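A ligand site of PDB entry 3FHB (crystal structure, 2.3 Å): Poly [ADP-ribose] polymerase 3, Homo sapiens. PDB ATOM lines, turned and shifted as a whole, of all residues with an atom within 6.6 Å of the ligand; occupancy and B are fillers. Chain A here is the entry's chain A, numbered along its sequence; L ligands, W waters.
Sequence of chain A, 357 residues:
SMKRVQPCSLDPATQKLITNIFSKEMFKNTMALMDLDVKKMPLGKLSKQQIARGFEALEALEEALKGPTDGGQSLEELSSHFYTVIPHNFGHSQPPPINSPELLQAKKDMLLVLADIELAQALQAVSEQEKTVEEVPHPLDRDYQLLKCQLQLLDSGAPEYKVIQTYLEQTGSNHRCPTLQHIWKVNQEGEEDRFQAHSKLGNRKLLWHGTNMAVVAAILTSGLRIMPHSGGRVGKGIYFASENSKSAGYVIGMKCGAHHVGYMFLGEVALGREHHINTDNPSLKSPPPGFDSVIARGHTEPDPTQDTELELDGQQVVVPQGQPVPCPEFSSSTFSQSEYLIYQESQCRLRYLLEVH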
ATOM      1  N   TRP A 208       2.098 -11.454 -22.321  1.00  0.00           N
ATOM      2  CA  TRP A 208       0.873 -12.055 -21.863  1.00  0.00           C
ATOM      3  C   TRP A 208       0.202 -12.734 -23.027  1.00  0.00           C
ATOM      4  O   TRP A 208       0.359 -12.313 -24.173  1.00  0.00           O
ATOM      5  CB  TRP A 208      -0.077 -10.985 -21.264  1.00  0.00           C
ATOM      6  CG  TRP A 208       0.468 -10.363 -20.006  1.00  0.00           C
ATOM      7  CD1 TRP A 208       1.015  -9.126 -19.872  1.00  0.00           C
ATOM      8  CD2 TRP A 208       0.546 -10.988 -18.716  1.00  0.00           C
ATOM      9  NE1 TRP A 208       1.429  -8.928 -18.564  1.00  0.00           N
ATOM     10  CE2 TRP A 208       1.164 -10.059 -17.839  1.00  0.00           C
ATOM     11  CE3 TRP A 208       0.164 -12.243 -18.216  1.00  0.00           C
ATOM     12  CZ2 TRP A 208       1.389 -10.334 -16.496  1.00  0.00           C
ATOM     13  CZ3 TRP A 208       0.381 -12.527 -16.866  1.00  0.00           C
ATOM     14  CH2 TRP A 208       1.000 -11.565 -16.017  1.00  0.00           C
ATOM     15  N   HIS A 209      -0.538 -13.798 -22.728  1.00  0.00           N
ATOM     16  CA  HIS A 209      -1.435 -14.414 -23.685  1.00  0.00           C
ATOM     17  C   HIS A 209      -2.587 -14.970 -22.888  1.00  0.00           C
ATOM     18  O   HIS A 209      -2.417 -15.951 -22.150  1.00  0.00           O
ATOM     19  CB  HIS A 209      -0.701 -15.520 -24.452  1.00  0.00           C
ATOM     20  CG  HIS A 209      -1.582 -16.273 -25.402  1.00  0.00           C
ATOM     21  ND1 HIS A 209      -1.804 -15.865 -26.697  1.00  0.00           N
ATOM     22  CD2 HIS A 209      -2.301 -17.402 -25.229  1.00  0.00           C
ATOM     23  CE1 HIS A 209      -2.642 -16.714 -27.284  1.00  0.00           C
ATOM     24  NE2 HIS A 209      -2.946 -17.665 -26.415  1.00  0.00           N
ATOM     25  N   GLY A 210      -3.740 -14.325 -22.999  1.00  0.00           N
ATOM     26  CA  GLY A 210      -4.977 -14.861 -22.419  1.00  0.00           C
ATOM     27  C   GLY A 210      -5.737 -15.792 -23.365  1.00  0.00           C
ATOM     28  O   GLY A 210      -5.734 -15.583 -24.575  1.00  0.00           O
ATOM     29  N   THR A 211      -6.397 -16.811 -22.800  1.00  0.00           N
ATOM     30  CA  THR A 211      -7.202 -17.772 -23.575  1.00  0.00           C
ATOM     31  C   THR A 211      -8.313 -18.271 -22.716  1.00  0.00           C
ATOM     32  O   THR A 211      -8.294 -18.077 -21.510  1.00  0.00           O
ATOM     33  CB  THR A 211      -6.449 -19.061 -23.869  1.00  0.00           C
ATOM     34  OG1 THR A 211      -5.996 -19.603 -22.617  1.00  0.00           O
ATOM     35  CG2 THR A 211      -5.304 -18.833 -24.799  1.00  0.00           C
ATOM     36  N   ARG A 233      -6.650  -9.105 -36.068  1.00  0.00           N
ATOM     37  CA  ARG A 233      -6.409  -7.781 -36.603  1.00  0.00           C
ATOM     38  C   ARG A 233      -5.010  -7.631 -37.168  1.00  0.00           C
ATOM     39  O   ARG A 233      -4.749  -6.652 -37.885  1.00  0.00           O
ATOM     40  CB  ARG A 233      -6.591  -6.725 -35.525  1.00  0.00           C
ATOM     41  CG  ARG A 233      -7.953  -6.615 -34.894  1.00  0.00           C
ATOM     42  CD  ARG A 233      -7.894  -5.570 -33.762  1.00  0.00           C
ATOM     43  NE  ARG A 233      -7.783  -4.190 -34.271  1.00  0.00           N
ATOM     44  CZ  ARG A 233      -7.707  -3.101 -33.518  1.00  0.00           C
ATOM     45  NH1 ARG A 233      -7.726  -3.161 -32.192  1.00  0.00           N
ATOM     46  NH2 ARG A 233      -7.625  -1.913 -34.094  1.00  0.00           N
ATOM     47  N   TYR A 239      -0.854 -14.203 -30.991  1.00  0.00           N
ATOM     48  CA  TYR A 239      -1.079 -12.916 -30.392  1.00  0.00           C
ATOM     49  C   TYR A 239      -0.643 -12.880 -28.939  1.00  0.00           C
ATOM     50  O   TYR A 239      -1.034 -13.765 -28.134  1.00  0.00           O
ATOM     51  CB  TYR A 239      -2.575 -12.599 -30.479  1.00  0.00           C
ATOM     52  CG  TYR A 239      -3.023 -12.268 -31.882  1.00  0.00           C
ATOM     53  CD1 TYR A 239      -3.254 -13.275 -32.836  1.00  0.00           C
ATOM     54  CD2 TYR A 239      -3.197 -10.940 -32.269  1.00  0.00           C
ATOM     55  CE1 TYR A 239      -3.675 -12.946 -34.130  1.00  0.00           C
ATOM     56  CE2 TYR A 239      -3.610 -10.602 -33.571  1.00  0.00           C
ATOM     57  CZ  TYR A 239      -3.828 -11.600 -34.487  1.00  0.00           C
ATOM     58  OH  TYR A 239      -4.208 -11.240 -35.752  1.00  0.00           O
ATOM     59  N   PHE A 240       0.150 -11.853 -28.627  1.00  0.00           N
ATOM     60  CA  PHE A 240       0.610 -11.556 -27.268  1.00  0.00           C
ATOM     61  C   PHE A 240       0.459 -10.075 -26.933  1.00  0.00           C
ATOM     62  O   PHE A 240       0.444  -9.219 -27.812  1.00  0.00           O
ATOM     63  CB  PHE A 240       2.083 -11.884 -27.098  1.00  0.00           C
ATOM     64  CG  PHE A 240       2.444 -13.300 -27.372  1.00  0.00           C
ATOM     65  CD1 PHE A 240       2.534 -14.229 -26.340  1.00  0.00           C
ATOM     66  CD2 PHE A 240       2.816 -13.692 -28.654  1.00  0.00           C
ATOM     67  CE1 PHE A 240       2.915 -15.538 -26.581  1.00  0.00           C
ATOM     68  CE2 PHE A 240       3.212 -14.982 -28.909  1.00  0.00           C
ATOM     69  CZ  PHE A 240       3.271 -15.917 -27.877  1.00  0.00           C
ATOM     70  N   ALA A 241       0.396  -9.750 -25.650  1.00  0.00           N
ATOM     71  CA  ALA A 241       0.289  -8.341 -25.222  1.00  0.00           C
ATOM     72  C   ALA A 241       1.268  -8.040 -24.108  1.00  0.00           C
ATOM     73  O   ALA A 241       1.522  -8.919 -23.274  1.00  0.00           O
ATOM     74  CB  ALA A 241      -1.150  -7.997 -24.803  1.00  0.00           C
ATOM     75  N   SER A 242       1.818  -6.810 -24.089  1.00  0.00           N
ATOM     76  CA  SER A 242       2.600  -6.290 -22.952  1.00  0.00           C
ATOM     77  C   SER A 242       1.708  -5.738 -21.848  1.00  0.00           C
ATOM     78  O   SER A 242       2.173  -5.504 -20.728  1.00  0.00           O
ATOM     79  CB  SER A 242       3.552  -5.175 -23.370  1.00  0.00           C
ATOM     80  OG  SER A 242       2.910  -4.214 -24.188  1.00  0.00           O
ATOM     81  N   GLU A 243       0.437  -5.525 -22.179  1.00  0.00           N
ATOM     82  CA  GLU A 243      -0.568  -5.112 -21.166  1.00  0.00           C
ATOM     83  C   GLU A 243      -1.514  -6.257 -20.793  1.00  0.00           C
ATOM     84  O   GLU A 243      -2.352  -6.682 -21.597  1.00  0.00           O
ATOM     85  CB  GLU A 243      -1.343  -3.877 -21.646  1.00  0.00           C
ATOM     86  CG  GLU A 243      -0.385  -2.726 -21.862  1.00  0.00           C
ATOM     87  CD  GLU A 243      -1.053  -1.404 -22.118  1.00  0.00           C
ATOM     88  OE1 GLU A 243      -1.978  -1.030 -21.369  1.00  0.00           O
ATOM     89  OE2 GLU A 243      -0.613  -0.722 -23.070  1.00  0.00           O
ATOM     90  N   LYS A 246      -5.097  -5.988 -21.661  1.00  0.00           N
ATOM     91  CA  LYS A 246      -5.435  -6.417 -23.040  1.00  0.00           C
ATOM     92  C   LYS A 246      -5.697  -7.918 -23.133  1.00  0.00           C
ATOM     93  O   LYS A 246      -6.717  -8.364 -23.667  1.00  0.00           O
ATOM     94  CB  LYS A 246      -4.326  -6.036 -24.036  1.00  0.00           C
ATOM     95  CG  LYS A 246      -4.570  -6.489 -25.481  1.00  0.00           C
ATOM     96  CD  LYS A 246      -5.812  -5.864 -26.068  1.00  0.00           C
ATOM     97  CE  LYS A 246      -5.996  -6.288 -27.523  1.00  0.00           C
ATOM     98  NZ  LYS A 246      -7.296  -5.839 -28.106  1.00  0.00           N
ATOM     99  N   SER A 247      -4.753  -8.711 -22.654  1.00  0.00           N
ATOM    100  CA  SER A 247      -4.885 -10.167 -22.673  1.00  0.00           C
ATOM    101  C   SER A 247      -6.036 -10.667 -21.777  1.00  0.00           C
ATOM    102  O   SER A 247      -6.621 -11.705 -22.070  1.00  0.00           O
ATOM    103  CB  SER A 247      -3.563 -10.833 -22.256  1.00  0.00           C
ATOM    104  OG  SER A 247      -2.590 -10.740 -23.295  1.00  0.00           O
ATOM    105  N   ALA A 248      -6.335  -9.940 -20.691  1.00  0.00           N
ATOM    106  CA  ALA A 248      -7.423 -10.327 -19.791  1.00  0.00           C
ATOM    107  C   ALA A 248      -8.767 -10.323 -20.530  1.00  0.00           C
ATOM    108  O   ALA A 248      -9.656 -11.143 -20.248  1.00  0.00           O
ATOM    109  CB  ALA A 248      -7.463  -9.419 -18.556  1.00  0.00           C
ATOM    110  N   TYR A 250      -9.321 -11.540 -23.296  1.00  0.00           N
ATOM    111  CA  TYR A 250      -9.480 -12.823 -24.028  1.00  0.00           C
ATOM    112  C   TYR A 250      -9.467 -14.046 -23.148  1.00  0.00           C
ATOM    113  O   TYR A 250      -9.522 -15.175 -23.630  1.00  0.00           O
ATOM    114  CB  TYR A 250      -8.383 -12.965 -25.093  1.00  0.00           C
ATOM    115  CG  TYR A 250      -8.361 -11.794 -26.028  1.00  0.00           C
ATOM    116  CD1 TYR A 250      -8.995 -11.841 -27.258  1.00  0.00           C
ATOM    117  CD2 TYR A 250      -7.712 -10.635 -25.665  1.00  0.00           C
ATOM    118  CE1 TYR A 250      -8.984 -10.756 -28.109  1.00  0.00           C
ATOM    119  CE2 TYR A 250      -7.695  -9.551 -26.495  1.00  0.00           C
ATOM    120  CZ  TYR A 250      -8.326  -9.607 -27.721  1.00  0.00           C
ATOM    121  OH  TYR A 250      -8.272  -8.487 -28.535  1.00  0.00           O
ATOM    122  N   VAL A 251      -9.362 -13.826 -21.843  1.00  0.00           N
ATOM    123  CA  VAL A 251      -9.503 -14.905 -20.880  1.00  0.00           C
ATOM    124  C   VAL A 251     -11.001 -15.151 -20.761  1.00  0.00           C
ATOM    125  O   VAL A 251     -11.772 -14.209 -20.635  1.00  0.00           O
ATOM    126  CB  VAL A 251      -8.943 -14.536 -19.475  1.00  0.00           C
ATOM    127  CG1 VAL A 251      -9.039 -15.731 -18.539  1.00  0.00           C
ATOM    128  CG2 VAL A 251      -7.484 -14.027 -19.564  1.00  0.00           C
ATOM    129  N   SER A 338      -0.905  -2.348 -27.530  1.00  0.00           N
ATOM    130  CA  SER A 338      -0.038  -3.064 -28.471  1.00  0.00           C
ATOM    131  C   SER A 338      -0.410  -4.567 -28.574  1.00  0.00           C
ATOM    132  O   SER A 338      -0.755  -5.203 -27.559  1.00  0.00           O
ATOM    133  CB  SER A 338       1.441  -2.889 -28.126  1.00  0.00           C
ATOM    134  OG  SER A 338       1.868  -1.544 -28.394  1.00  0.00           O
ATOM    135  N   GLU A 339      -0.387  -5.086 -29.803  1.00  0.00           N
ATOM    136  CA  GLU A 339      -0.543  -6.515 -30.074  1.00  0.00           C
ATOM    137  C   GLU A 339       0.769  -7.002 -30.659  1.00  0.00           C
ATOM    138  O   GLU A 339       1.195  -6.494 -31.694  1.00  0.00           O
ATOM    139  CB  GLU A 339      -1.703  -6.790 -31.036  1.00  0.00           C
ATOM    140  CG  GLU A 339      -3.043  -6.127 -30.614  1.00  0.00           C
ATOM    141  CD  GLU A 339      -4.303  -6.726 -31.271  1.00  0.00           C
ATOM    142  OE1 GLU A 339      -4.200  -7.635 -32.140  1.00  0.00           O
ATOM    143  OE2 GLU A 339      -5.407  -6.282 -30.885  1.00  0.00           O
ATOM    144  N   TYR A 340       1.409  -7.956 -29.997  1.00  0.00           N
ATOM    145  CA  TYR A 340       2.706  -8.473 -30.445  1.00  0.00           C
ATOM    146  C   TYR A 340       2.475  -9.760 -31.232  1.00  0.00           C
ATOM    147  O   TYR A 340       1.829 -10.687 -30.742  1.00  0.00           O
ATOM    148  CB  TYR A 340       3.621  -8.782 -29.279  1.00  0.00           C
ATOM    149  CG  TYR A 340       4.180  -7.559 -28.591  1.00  0.00           C
ATOM    150  CD1 TYR A 340       3.347  -6.696 -27.878  1.00  0.00           C
ATOM    151  CD2 TYR A 340       5.546  -7.277 -28.627  1.00  0.00           C
ATOM    152  CE1 TYR A 340       3.842  -5.571 -27.258  1.00  0.00           C
ATOM    153  CE2 TYR A 340       6.068  -6.139 -27.989  1.00  0.00           C
ATOM    154  CZ  TYR A 340       5.206  -5.293 -27.304  1.00  0.00           C
ATOM    155  OH  TYR A 340       5.688  -4.191 -26.657  1.00  0.00           O
ATOM    156  N   LEU A 341       3.022  -9.810 -32.443  1.00  0.00           N
ATOM    157  CA  LEU A 341       2.805 -10.929 -33.332  1.00  0.00           C
ATOM    158  C   LEU A 341       4.090 -11.594 -33.759  1.00  0.00           C
ATOM    159  O   LEU A 341       5.025 -10.939 -34.229  1.00  0.00           O
ATOM    160  CB  LEU A 341       2.045 -10.477 -34.589  1.00  0.00           C
ATOM    161  CG  LEU A 341       0.515 -10.418 -34.544  1.00  0.00           C
ATOM    162  CD1 LEU A 341      -0.104 -11.837 -34.560  1.00  0.00           C
ATOM    163  CD2 LEU A 341       0.036  -9.601 -33.361  1.00  0.00           C
HETATM  164  C1  LIG L   1      -4.161 -12.533 -26.073  1.00  0.00           C
HETATM  165  O1  LIG L   1      -3.756 -12.368 -24.886  1.00  0.00           O
HETATM  166  O2  LIG L   1      -4.669 -13.593 -26.544  1.00  0.00           O
HETATM  167  C2  LIG L   1      -4.021 -11.364 -27.034  1.00  0.00           C
HETATM  168  C3  LIG L   1      -4.905 -11.221 -28.090  1.00  0.00           C
HETATM  169  C4  LIG L   1      -4.732 -10.138 -28.960  1.00  0.00           C
HETATM  170  C5  LIG L   1      -3.707  -9.230 -28.781  1.00  0.00           C
HETATM  171  C6  LIG L   1      -2.841  -9.395 -27.719  1.00  0.00           C
HETATM  172  C7  LIG L   1      -2.996 -10.456 -26.855  1.00  0.00           C
HETATM  173  N1  LIG L   1      -5.559  -9.964 -29.969  1.00  0.00           N
HETATM  174  O   HOH W   1      -6.715  -9.232 -33.006  1.00  0.00           O
HETATM  175  O   HOH W   2      -5.978 -14.912 -29.113  1.00  0.00           O
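The backbone carbonyl oxygen (O) of Trp 208 lies close to the side-chain hydroxyl (OG) of Ser 247, at 3.5 Å.
The backbone carbonyl oxygen (O) of Phe 240 lies within hydrogen-bond range of the backbone NH (N) of Tyr 340 (2.7 Å).
A ring nitrogen (ND1) of His 209 is in hydrogen-bond range of the backbone carbonyl oxygen (O) of Tyr 239 (2.7 Å).
OH of Tyr 250 sits at hydrogen-bond distance from NZ of Lys 246 (2.9 Å).
The backbone NH of Arg 233 is in hydrogen-bond range of the side-chain hydroxyl of Tyr 239, at 3.3 Å.
The side-chain carboxylate (OE2) of Glu 339 lies within salt-bridge range of the side-chain amino group (NZ) of Lys 246, 3.4 Å away.
N of Trp 208 sits at hydrogen-bond distance from O of Ala 241 (2.8 Å).
Merely in contact with the ligand: Phe 240 (3.3 Å), His 209 (3.3 Å), Tyr 239 (3.4 Å), Ala 241 (3.6 Å) and Lys 246 (3.9 Å).
Water W1 lies within hydrogen-bond range of the backbone NH (N) of Arg 233 (3.1 Å), the side-chain carboxylate (OE1) of Glu 339 (3.1 Å) and a nitrogen (N1) of the ligand (3.3 Å).
An oxygen (O1) of the ligand sits at hydrogen-bond distance from the side-chain hydroxyl (OG) of Ser 247.
The backbone NH (N) of Gly 210 is in hydrogen-bond range of an oxygen (O1) of the ligand (2.7 Å).
The backbone carbonyl oxygen of Gly 210 sits close to an oxygen (O2) of the ligand.
The side-chain hydroxyl (OH) of Tyr 250 is in hydrogen-bond range of a nitrogen (N1) of the ligand (3.4 Å).
A nitrogen (N1) of the ligand sits at hydrogen-bond distance from the side-chain carboxylate (OE1) of Glu 339 (3.5 Å).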
